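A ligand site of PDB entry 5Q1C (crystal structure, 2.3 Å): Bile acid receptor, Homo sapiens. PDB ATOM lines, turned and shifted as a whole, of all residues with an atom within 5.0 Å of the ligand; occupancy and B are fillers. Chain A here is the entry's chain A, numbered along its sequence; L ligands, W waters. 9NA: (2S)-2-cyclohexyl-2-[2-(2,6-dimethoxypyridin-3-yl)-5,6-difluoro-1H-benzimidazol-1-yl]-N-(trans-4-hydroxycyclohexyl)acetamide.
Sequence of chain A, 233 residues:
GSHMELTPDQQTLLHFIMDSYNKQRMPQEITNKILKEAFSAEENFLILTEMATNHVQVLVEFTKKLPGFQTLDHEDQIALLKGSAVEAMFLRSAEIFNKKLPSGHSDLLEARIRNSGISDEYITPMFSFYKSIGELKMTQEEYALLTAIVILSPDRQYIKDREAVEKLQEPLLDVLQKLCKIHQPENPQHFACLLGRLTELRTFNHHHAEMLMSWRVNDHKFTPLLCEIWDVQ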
ATOM      1  N   ILE A  30     -25.480 -15.795  16.158  1.00  0.00           N
ATOM      2  CA  ILE A  30     -24.986 -16.984  15.478  1.00  0.00           C
ATOM      3  C   ILE A  30     -25.820 -18.237  15.845  1.00  0.00           C
ATOM      4  O   ILE A  30     -26.288 -18.926  14.945  1.00  0.00           O
ATOM      5  CB  ILE A  30     -23.451 -17.146  15.747  1.00  0.00           C
ATOM      6  CG1 ILE A  30     -22.655 -16.036  15.029  1.00  0.00           C
ATOM      7  CG2 ILE A  30     -22.916 -18.522  15.346  1.00  0.00           C
ATOM      8  CD1 ILE A  30     -22.079 -15.034  15.879  1.00  0.00           C
ATOM      9  N   THR A  31     -25.993 -18.505  17.161  1.00  0.00           N
ATOM     10  CA  THR A  31     -26.730 -19.669  17.676  1.00  0.00           C
ATOM     11  C   THR A  31     -28.218 -19.612  17.356  1.00  0.00           C
ATOM     12  O   THR A  31     -28.825 -20.669  17.208  1.00  0.00           O
ATOM     13  CB  THR A  31     -26.487 -19.906  19.152  1.00  0.00           C
ATOM     14  OG1 THR A  31     -26.858 -18.730  19.886  1.00  0.00           O
ATOM     15  CG2 THR A  31     -25.061 -20.339  19.442  1.00  0.00           C
ATOM     16  N   ILE A  34     -28.562 -20.980  13.609  1.00  0.00           N
ATOM     17  CA  ILE A  34     -28.333 -22.430  13.545  1.00  0.00           C
ATOM     18  C   ILE A  34     -29.488 -23.223  14.187  1.00  0.00           C
ATOM     19  O   ILE A  34     -29.950 -24.193  13.593  1.00  0.00           O
ATOM     20  CB  ILE A  34     -26.924 -22.814  14.127  1.00  0.00           C
ATOM     21  CG1 ILE A  34     -25.785 -22.004  13.449  1.00  0.00           C
ATOM     22  CG2 ILE A  34     -26.663 -24.334  14.049  1.00  0.00           C
ATOM     23  CD1 ILE A  34     -24.462 -21.949  14.232  1.00  0.00           C
ATOM     24  N   ASN A  44     -25.361 -24.059   4.602  1.00  0.00           N
ATOM     25  CA  ASN A  44     -24.409 -24.013   5.717  1.00  0.00           C
ATOM     26  C   ASN A  44     -23.015 -23.571   5.284  1.00  0.00           C
ATOM     27  O   ASN A  44     -22.358 -22.877   6.062  1.00  0.00           O
ATOM     28  CB  ASN A  44     -24.372 -25.342   6.456  1.00  0.00           C
ATOM     29  CG  ASN A  44     -25.536 -25.565   7.392  1.00  0.00           C
ATOM     30  OD1 ASN A  44     -26.050 -24.635   8.037  1.00  0.00           O
ATOM     31  ND2 ASN A  44     -25.959 -26.822   7.521  1.00  0.00           N
ATOM     32  N   ILE A  47     -23.336 -19.851   4.872  1.00  0.00           N
ATOM     33  CA  ILE A  47     -23.442 -19.251   6.209  1.00  0.00           C
ATOM     34  C   ILE A  47     -22.019 -19.142   6.789  1.00  0.00           C
ATOM     35  O   ILE A  47     -21.638 -18.067   7.255  1.00  0.00           O
ATOM     36  CB  ILE A  47     -24.431 -20.056   7.129  1.00  0.00           C
ATOM     37  CG1 ILE A  47     -25.902 -19.853   6.681  1.00  0.00           C
ATOM     38  CG2 ILE A  47     -24.261 -19.683   8.618  1.00  0.00           C
ATOM     39  CD1 ILE A  47     -26.895 -20.951   7.154  1.00  0.00           C
ATOM     40  N   LEU A  48     -21.218 -20.220   6.669  1.00  0.00           N
ATOM     41  CA  LEU A  48     -19.837 -20.275   7.148  1.00  0.00           C
ATOM     42  C   LEU A  48     -18.894 -19.252   6.483  1.00  0.00           C
ATOM     43  O   LEU A  48     -18.132 -18.600   7.195  1.00  0.00           O
ATOM     44  CB  LEU A  48     -19.256 -21.703   7.040  1.00  0.00           C
ATOM     45  CG  LEU A  48     -17.745 -21.884   7.374  1.00  0.00           C
ATOM     46  CD1 LEU A  48     -17.457 -21.627   8.856  1.00  0.00           C
ATOM     47  CD2 LEU A  48     -17.253 -23.246   6.963  1.00  0.00           C
ATOM     48  N   MET A  51     -19.910 -15.758   7.701  1.00  0.00           N
ATOM     49  CA  MET A  51     -19.500 -15.642   9.113  1.00  0.00           C
ATOM     50  C   MET A  51     -17.999 -15.428   9.217  1.00  0.00           C
ATOM     51  O   MET A  51     -17.549 -14.588   9.987  1.00  0.00           O
ATOM     52  CB  MET A  51     -19.873 -16.914   9.916  1.00  0.00           C
ATOM     53  CG  MET A  51     -21.340 -17.031  10.203  1.00  0.00           C
ATOM     54  SD  MET A  51     -21.888 -15.883  11.460  1.00  0.00           S
ATOM     55  CE  MET A  51     -23.654 -16.070  11.262  1.00  0.00           C
ATOM     56  N   ALA A  52     -17.212 -16.188   8.439  1.00  0.00           N
ATOM     57  CA  ALA A  52     -15.755 -16.116   8.399  1.00  0.00           C
ATOM     58  C   ALA A  52     -15.234 -14.825   7.757  1.00  0.00           C
ATOM     59  O   ALA A  52     -14.146 -14.369   8.133  1.00  0.00           O
ATOM     60  CB  ALA A  52     -15.188 -17.327   7.701  1.00  0.00           C
ATOM     61  N   ASN A  54     -16.909 -11.908   7.909  1.00  0.00           N
ATOM     62  CA  ASN A  54     -17.167 -10.921   8.961  1.00  0.00           C
ATOM     63  C   ASN A  54     -16.095 -11.024  10.051  1.00  0.00           C
ATOM     64  O   ASN A  54     -15.557  -9.994  10.463  1.00  0.00           O
ATOM     65  CB  ASN A  54     -18.569 -11.111   9.553  1.00  0.00           C
ATOM     66  CG  ASN A  54     -18.804 -10.342  10.824  1.00  0.00           C
ATOM     67  OD1 ASN A  54     -19.132  -9.161  10.832  1.00  0.00           O
ATOM     68  ND2 ASN A  54     -18.600 -10.979  11.942  1.00  0.00           N
ATOM     69  N   HIS A  55     -15.763 -12.259  10.488  1.00  0.00           N
ATOM     70  CA  HIS A  55     -14.756 -12.524  11.516  1.00  0.00           C
ATOM     71  C   HIS A  55     -13.405 -11.904  11.185  1.00  0.00           C
ATOM     72  O   HIS A  55     -12.824 -11.236  12.039  1.00  0.00           O
ATOM     73  CB  HIS A  55     -14.625 -14.025  11.809  1.00  0.00           C
ATOM     74  CG  HIS A  55     -13.542 -14.315  12.796  1.00  0.00           C
ATOM     75  ND1 HIS A  55     -13.755 -14.157  14.159  1.00  0.00           N
ATOM     76  CD2 HIS A  55     -12.271 -14.693  12.619  1.00  0.00           C
ATOM     77  CE1 HIS A  55     -12.624 -14.455  14.751  1.00  0.00           C
ATOM     78  NE2 HIS A  55     -11.698 -14.753  13.887  1.00  0.00           N
ATOM     79  N   MET A  89     -10.600 -17.722  14.760  1.00  0.00           N
ATOM     80  CA  MET A  89     -11.940 -18.127  14.340  1.00  0.00           C
ATOM     81  C   MET A  89     -12.420 -19.343  15.128  1.00  0.00           C
ATOM     82  O   MET A  89     -13.543 -19.328  15.611  1.00  0.00           O
ATOM     83  CB  MET A  89     -11.961 -18.388  12.825  1.00  0.00           C
ATOM     84  CG  MET A  89     -13.309 -18.822  12.308  1.00  0.00           C
ATOM     85  SD  MET A  89     -13.300 -19.307  10.587  1.00  0.00           S
ATOM     86  CE  MET A  89     -12.100 -20.724  10.642  1.00  0.00           C
ATOM     87  N   PHE A  90     -11.566 -20.370  15.262  1.00  0.00           N
ATOM     88  CA  PHE A  90     -11.879 -21.582  16.025  1.00  0.00           C
ATOM     89  C   PHE A  90     -12.008 -21.312  17.512  1.00  0.00           C
ATOM     90  O   PHE A  90     -12.847 -21.929  18.146  1.00  0.00           O
ATOM     91  CB  PHE A  90     -10.867 -22.716  15.742  1.00  0.00           C
ATOM     92  CG  PHE A  90     -11.198 -23.482  14.475  1.00  0.00           C
ATOM     93  CD1 PHE A  90     -12.220 -24.430  14.462  1.00  0.00           C
ATOM     94  CD2 PHE A  90     -10.506 -23.233  13.300  1.00  0.00           C
ATOM     95  CE1 PHE A  90     -12.538 -25.112  13.287  1.00  0.00           C
ATOM     96  CE2 PHE A  90     -10.825 -23.923  12.130  1.00  0.00           C
ATOM     97  CZ  PHE A  90     -11.835 -24.863  12.134  1.00  0.00           C
ATOM     98  N   ARG A  92     -13.036 -18.406  18.853  1.00  0.00           N
ATOM     99  CA  ARG A  92     -14.317 -17.707  18.917  1.00  0.00           C
ATOM    100  C   ARG A  92     -15.499 -18.684  18.825  1.00  0.00           C
ATOM    101  O   ARG A  92     -16.479 -18.537  19.544  1.00  0.00           O
ATOM    102  CB  ARG A  92     -14.429 -16.624  17.816  1.00  0.00           C
ATOM    103  CG  ARG A  92     -15.678 -15.757  17.860  1.00  0.00           C
ATOM    104  CD  ARG A  92     -15.969 -15.154  19.231  1.00  0.00           C
ATOM    105  NE  ARG A  92     -17.165 -14.317  19.194  1.00  0.00           N
ATOM    106  CZ  ARG A  92     -17.674 -13.680  20.250  1.00  0.00           C
ATOM    107  NH1 ARG A  92     -17.105 -13.794  21.440  1.00  0.00           N
ATOM    108  NH2 ARG A  92     -18.740 -12.910  20.111  1.00  0.00           N
ATOM    109  N   SER A  93     -15.398 -19.698  17.946  1.00  0.00           N
ATOM    110  CA  SER A  93     -16.408 -20.743  17.742  1.00  0.00           C
ATOM    111  C   SER A  93     -16.523 -21.556  19.031  1.00  0.00           C
ATOM    112  O   SER A  93     -17.645 -21.869  19.444  1.00  0.00           O
ATOM    113  CB  SER A  93     -16.018 -21.638  16.581  1.00  0.00           C
ATOM    114  OG  SER A  93     -16.046 -20.933  15.346  1.00  0.00           O
ATOM    115  N   ILE A  96     -18.475 -19.420  21.706  1.00  0.00           N
ATOM    116  CA  ILE A  96     -19.903 -19.451  21.349  1.00  0.00           C
ATOM    117  C   ILE A  96     -20.490 -20.819  21.689  1.00  0.00           C
ATOM    118  O   ILE A  96     -21.560 -20.879  22.260  1.00  0.00           O
ATOM    119  CB  ILE A  96     -20.116 -19.055  19.857  1.00  0.00           C
ATOM    120  CG1 ILE A  96     -19.659 -17.599  19.576  1.00  0.00           C
ATOM    121  CG2 ILE A  96     -21.574 -19.223  19.432  1.00  0.00           C
ATOM    122  CD1 ILE A  96     -19.329 -17.294  18.123  1.00  0.00           C
ATOM    123  N   PHE A  97     -19.780 -21.912  21.389  1.00  0.00           N
ATOM    124  CA  PHE A  97     -20.231 -23.275  21.695  1.00  0.00           C
ATOM    125  C   PHE A  97     -20.469 -23.503  23.189  1.00  0.00           C
ATOM    126  O   PHE A  97     -21.455 -24.148  23.543  1.00  0.00           O
ATOM    127  CB  PHE A  97     -19.233 -24.308  21.153  1.00  0.00           C
ATOM    128  CG  PHE A  97     -19.712 -25.746  21.211  1.00  0.00           C
ATOM    129  CD1 PHE A  97     -20.573 -26.254  20.249  1.00  0.00           C
ATOM    130  CD2 PHE A  97     -19.282 -26.595  22.225  1.00  0.00           C
ATOM    131  CE1 PHE A  97     -21.010 -27.584  20.305  1.00  0.00           C
ATOM    132  CE2 PHE A  97     -19.701 -27.933  22.272  1.00  0.00           C
ATOM    133  CZ  PHE A  97     -20.560 -28.413  21.320  1.00  0.00           C
ATOM    134  N   LEU A 109     -27.628 -27.747  18.934  1.00  0.00           N
ATOM    135  CA  LEU A 109     -26.583 -26.975  18.285  1.00  0.00           C
ATOM    136  C   LEU A 109     -25.440 -27.906  17.846  1.00  0.00           C
ATOM    137  O   LEU A 109     -25.007 -27.819  16.697  1.00  0.00           O
ATOM    138  CB  LEU A 109     -26.068 -25.865  19.227  1.00  0.00           C
ATOM    139  CG  LEU A 109     -24.939 -24.950  18.695  1.00  0.00           C
ATOM    140  CD1 LEU A 109     -25.464 -23.956  17.642  1.00  0.00           C
ATOM    141  CD2 LEU A 109     -24.280 -24.206  19.832  1.00  0.00           C
ATOM    142  N   ILE A 113     -24.355 -28.727  14.011  1.00  0.00           N
ATOM    143  CA  ILE A 113     -22.971 -28.543  13.550  1.00  0.00           C
ATOM    144  C   ILE A 113     -22.438 -29.863  12.957  1.00  0.00           C
ATOM    145  O   ILE A 113     -21.856 -29.845  11.875  1.00  0.00           O
ATOM    146  CB  ILE A 113     -22.025 -27.913  14.630  1.00  0.00           C
ATOM    147  CG1 ILE A 113     -22.544 -26.527  15.119  1.00  0.00           C
ATOM    148  CG2 ILE A 113     -20.588 -27.771  14.109  1.00  0.00           C
ATOM    149  CD1 ILE A 113     -22.059 -26.115  16.482  1.00  0.00           C
ATOM    150  N   SER A 116     -23.694 -30.255   9.446  1.00  0.00           N
ATOM    151  CA  SER A 116     -23.596 -29.019   8.682  1.00  0.00           C
ATOM    152  C   SER A 116     -23.157 -29.220   7.227  1.00  0.00           C
ATOM    153  O   SER A 116     -23.622 -28.500   6.346  1.00  0.00           O
ATOM    154  CB  SER A 116     -22.705 -27.998   9.391  1.00  0.00           C
ATOM    155  OG  SER A 116     -21.371 -28.455   9.466  1.00  0.00           O
ATOM    156  N   ILE A 118     -19.595 -30.678   6.894  1.00  0.00           N
ATOM    157  CA  ILE A 118     -18.201 -31.040   7.199  1.00  0.00           C
ATOM    158  C   ILE A 118     -18.053 -32.573   7.315  1.00  0.00           C
ATOM    159  O   ILE A 118     -18.947 -33.233   7.856  1.00  0.00           O
ATOM    160  CB  ILE A 118     -17.713 -30.260   8.455  1.00  0.00           C
ATOM    161  CG1 ILE A 118     -16.213 -30.468   8.717  1.00  0.00           C
ATOM    162  CG2 ILE A 118     -18.555 -30.562   9.699  1.00  0.00           C
ATOM    163  CD1 ILE A 118     -15.536 -29.302   9.330  1.00  0.00           C
ATOM    164  N   MET A 126     -12.637 -31.390  16.480  1.00  0.00           N
ATOM    165  CA  MET A 126     -13.253 -30.068  16.636  1.00  0.00           C
ATOM    166  C   MET A 126     -14.089 -30.017  17.911  1.00  0.00           C
ATOM    167  O   MET A 126     -13.965 -29.065  18.684  1.00  0.00           O
ATOM    168  CB  MET A 126     -14.097 -29.740  15.415  1.00  0.00           C
ATOM    169  CG  MET A 126     -14.547 -28.298  15.357  1.00  0.00           C
ATOM    170  SD  MET A 126     -15.401 -27.903  13.818  1.00  0.00           S
ATOM    171  CE  MET A 126     -16.906 -28.796  14.029  1.00  0.00           C
ATOM    172  N   TYR A 130     -13.475 -28.018  21.564  1.00  0.00           N
ATOM    173  CA  TYR A 130     -14.583 -27.213  22.099  1.00  0.00           C
ATOM    174  C   TYR A 130     -14.907 -27.623  23.529  1.00  0.00           C
ATOM    175  O   TYR A 130     -14.965 -26.762  24.417  1.00  0.00           O
ATOM    176  CB  TYR A 130     -15.845 -27.345  21.215  1.00  0.00           C
ATOM    177  CG  TYR A 130     -15.767 -26.693  19.854  1.00  0.00           C
ATOM    178  CD1 TYR A 130     -14.693 -25.876  19.501  1.00  0.00           C
ATOM    179  CD2 TYR A 130     -16.782 -26.870  18.922  1.00  0.00           C
ATOM    180  CE1 TYR A 130     -14.629 -25.262  18.254  1.00  0.00           C
ATOM    181  CE2 TYR A 130     -16.714 -26.289  17.658  1.00  0.00           C
ATOM    182  CZ  TYR A 130     -15.649 -25.465  17.337  1.00  0.00           C
ATOM    183  OH  TYR A 130     -15.565 -24.871  16.102  1.00  0.00           O
ATOM    184  N   MET A 211     -10.614 -29.125   5.503  1.00  0.00           N
ATOM    185  CA  MET A 211     -11.922 -29.061   6.185  1.00  0.00           C
ATOM    186  C   MET A 211     -12.957 -28.423   5.278  1.00  0.00           C
ATOM    187  O   MET A 211     -14.073 -28.936   5.144  1.00  0.00           O
ATOM    188  CB  MET A 211     -11.840 -28.209   7.471  1.00  0.00           C
ATOM    189  CG  MET A 211     -11.391 -28.961   8.685  1.00  0.00           C
ATOM    190  SD  MET A 211     -11.226 -27.825  10.089  1.00  0.00           S
ATOM    191  CE  MET A 211     -12.444 -28.456  11.149  1.00  0.00           C
ATOM    192  N   LEU A 212     -12.556 -27.311   4.631  1.00  0.00           N
ATOM    193  CA  LEU A 212     -13.385 -26.547   3.700  1.00  0.00           C
ATOM    194  C   LEU A 212     -13.618 -27.249   2.388  1.00  0.00           C
ATOM    195  O   LEU A 212     -14.759 -27.243   1.915  1.00  0.00           O
ATOM    196  CB  LEU A 212     -12.776 -25.173   3.441  1.00  0.00           C
ATOM    197  CG  LEU A 212     -12.636 -24.287   4.661  1.00  0.00           C
ATOM    198  CD1 LEU A 212     -11.493 -23.365   4.497  1.00  0.00           C
ATOM    199  CD2 LEU A 212     -13.939 -23.573   4.994  1.00  0.00           C
ATOM    200  N   TRP A 215     -16.083 -30.343   2.412  1.00  0.00           N
ATOM    201  CA  TRP A 215     -17.477 -30.015   2.690  1.00  0.00           C
ATOM    202  C   TRP A 215     -18.382 -30.635   1.617  1.00  0.00           C
ATOM    203  O   TRP A 215     -18.002 -30.624   0.440  1.00  0.00           O
ATOM    204  CB  TRP A 215     -17.666 -28.495   2.706  1.00  0.00           C
ATOM    205  CG  TRP A 215     -18.859 -28.040   3.500  1.00  0.00           C
ATOM    206  CD1 TRP A 215     -20.158 -28.028   3.093  1.00  0.00           C
ATOM    207  CD2 TRP A 215     -18.845 -27.519   4.835  1.00  0.00           C
ATOM    208  NE1 TRP A 215     -20.962 -27.535   4.093  1.00  0.00           N
ATOM    209  CE2 TRP A 215     -20.181 -27.210   5.179  1.00  0.00           C
ATOM    210  CE3 TRP A 215     -17.835 -27.318   5.788  1.00  0.00           C
ATOM    211  CZ2 TRP A 215     -20.528 -26.698   6.433  1.00  0.00           C
ATOM    212  CZ3 TRP A 215     -18.186 -26.812   7.030  1.00  0.00           C
ATOM    213  CH2 TRP A 215     -19.516 -26.488   7.340  1.00  0.00           C
HETATM  214  N3  9NA L   1     -18.049 -24.251  14.772  1.00  0.00           N
HETATM  215  C4  9NA L   1     -19.737 -22.725  14.621  1.00  0.00           C
HETATM  216  C5  9NA L   1     -17.310 -24.377  12.417  1.00  0.00           C
HETATM  217  C6  9NA L   1     -19.030 -23.545  15.477  1.00  0.00           C
HETATM  218  C7  9NA L   1     -19.596 -20.765  12.159  1.00  0.00           C
HETATM  219  C8  9NA L   1     -16.202 -23.670  11.898  1.00  0.00           C
HETATM  220  C10 9NA L   1     -19.543 -22.316  12.025  1.00  0.00           C
HETATM  221  C15 9NA L   1     -20.364 -22.776  17.272  1.00  0.00           C
HETATM  222  C17 9NA L   1     -15.715 -25.309  10.385  1.00  0.00           C
HETATM  223  C20 9NA L   1     -16.787 -26.109  10.810  1.00  0.00           C
HETATM  224  C22 9NA L   1     -18.374 -18.782  13.053  1.00  0.00           C
HETATM  225  C26 9NA L   1     -17.532 -16.297  14.446  1.00  0.00           C
HETATM  226  C28 9NA L   1     -16.905 -18.396  13.103  1.00  0.00           C
HETATM  227  C1  9NA L   1     -18.168 -23.864  13.520  1.00  0.00           C
HETATM  228  N2  9NA L   1     -19.180 -22.947  13.348  1.00  0.00           N
HETATM  229  C12 9NA L   1     -19.337 -23.583  16.835  1.00  0.00           C
HETATM  230  C14 9NA L   1     -21.068 -21.969  16.414  1.00  0.00           C
HETATM  231  C11 9NA L   1     -20.783 -21.910  15.067  1.00  0.00           C
HETATM  232  F23 9NA L   1     -22.073 -21.195  16.903  1.00  0.00           F
HETATM  233  F24 9NA L   1     -20.691 -22.783  18.596  1.00  0.00           F
HETATM  234  O18 9NA L   1     -20.517 -20.101  11.705  1.00  0.00           O
HETATM  235  N13 9NA L   1     -18.546 -20.218  12.810  1.00  0.00           N
HETATM  236  C27 9NA L   1     -19.081 -18.322  14.312  1.00  0.00           C
HETATM  237  C29 9NA L   1     -18.999 -16.805  14.466  1.00  0.00           C
HETATM  238  C30 9NA L   1     -16.705 -16.877  13.254  1.00  0.00           C
HETATM  239  O31 9NA L   1     -17.545 -14.869  14.369  1.00  0.00           O
HETATM  240  C19 9NA L   1     -20.625 -23.138  11.286  1.00  0.00           C
HETATM  241  C32 9NA L   1     -21.639 -23.809  12.209  1.00  0.00           C
HETATM  242  C36 9NA L   1     -22.503 -24.806  11.448  1.00  0.00           C
HETATM  243  C38 9NA L   1     -23.236 -24.151  10.267  1.00  0.00           C
HETATM  244  C37 9NA L   1     -22.258 -23.306   9.354  1.00  0.00           C
HETATM  245  C33 9NA L   1     -21.351 -22.363  10.196  1.00  0.00           C
HETATM  246  N9  9NA L   1     -15.427 -24.114  10.914  1.00  0.00           N
HETATM  247  C16 9NA L   1     -17.583 -25.626  11.837  1.00  0.00           C
HETATM  248  O25 9NA L   1     -14.941 -25.802   9.376  1.00  0.00           O
HETATM  249  C35 9NA L   1     -14.175 -24.890   8.604  1.00  0.00           C
HETATM  250  O21 9NA L   1     -15.950 -22.480  12.448  1.00  0.00           O
HETATM  251  C34 9NA L   1     -14.642 -22.255  12.953  1.00  0.00           C
HETATM  252  O   HOH W   1     -18.670 -13.654  12.268  1.00  0.00           O
HETATM  253  O   HOH W   2     -16.152 -12.472  15.454  1.00  0.00           O
HETATM  254  O   HOH W   3     -18.686 -13.738  16.768  1.00  0.00           O
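OH of Tyr 130 sits at hydrogen-bond distance from N3 of the ligand, 2.9 Å away.
The side-chain hydroxyl (OG) of Ser 93 sits close to an oxygen (O21) of the ligand (3.3 Å).
The backbone carbonyl oxygen (O) of Ile 113 sits at hydrogen-bond distance from the side-chain hydroxyl (OG) of Ser 116, 2.8 Å away.
OG of Ser 93 sits at hydrogen-bond distance from O of Met 89 (3.0 Å).
The side-chain hydroxyl (OH) of Tyr 130 lies close to the side-chain sulfur (SD) of Met 126 (3.8 Å).
NE2 of His 55 is in hydrogen-bond range of N of Met 89 (3.3 Å).
The backbone carbonyl oxygen (O) of Ser 116 lies within hydrogen-bond range of the side-chain amide nitrogen (ND2) of Asn 44.
F24 of the ligand sits close to N of Phe 97 (3.1 Å).
Residues that only touch the ligand: Ile 30, Ile 34, Asn 44, Leu 48, Met 51, His 55, Met 89, Phe 90, Arg 92, Ile 96, Ile 113, Ser 116, Ile 118, Met 126 and Leu 212.
Water W1 lies within hydrogen-bond range of an oxygen (O31) of the ligand, the side-chain amide nitrogen of Asn 54 and the backbone carbonyl oxygen of Met 51.
Water W3 lies within hydrogen-bond range of an oxygen (O31) of the ligand (2.9 Å) and the guanidinium group of Arg 92 (2.9 Å).
Water W2 lies within hydrogen-bond range of O31 of the ligand (3.0 Å) and ND1 of His 55 (3.2 Å).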
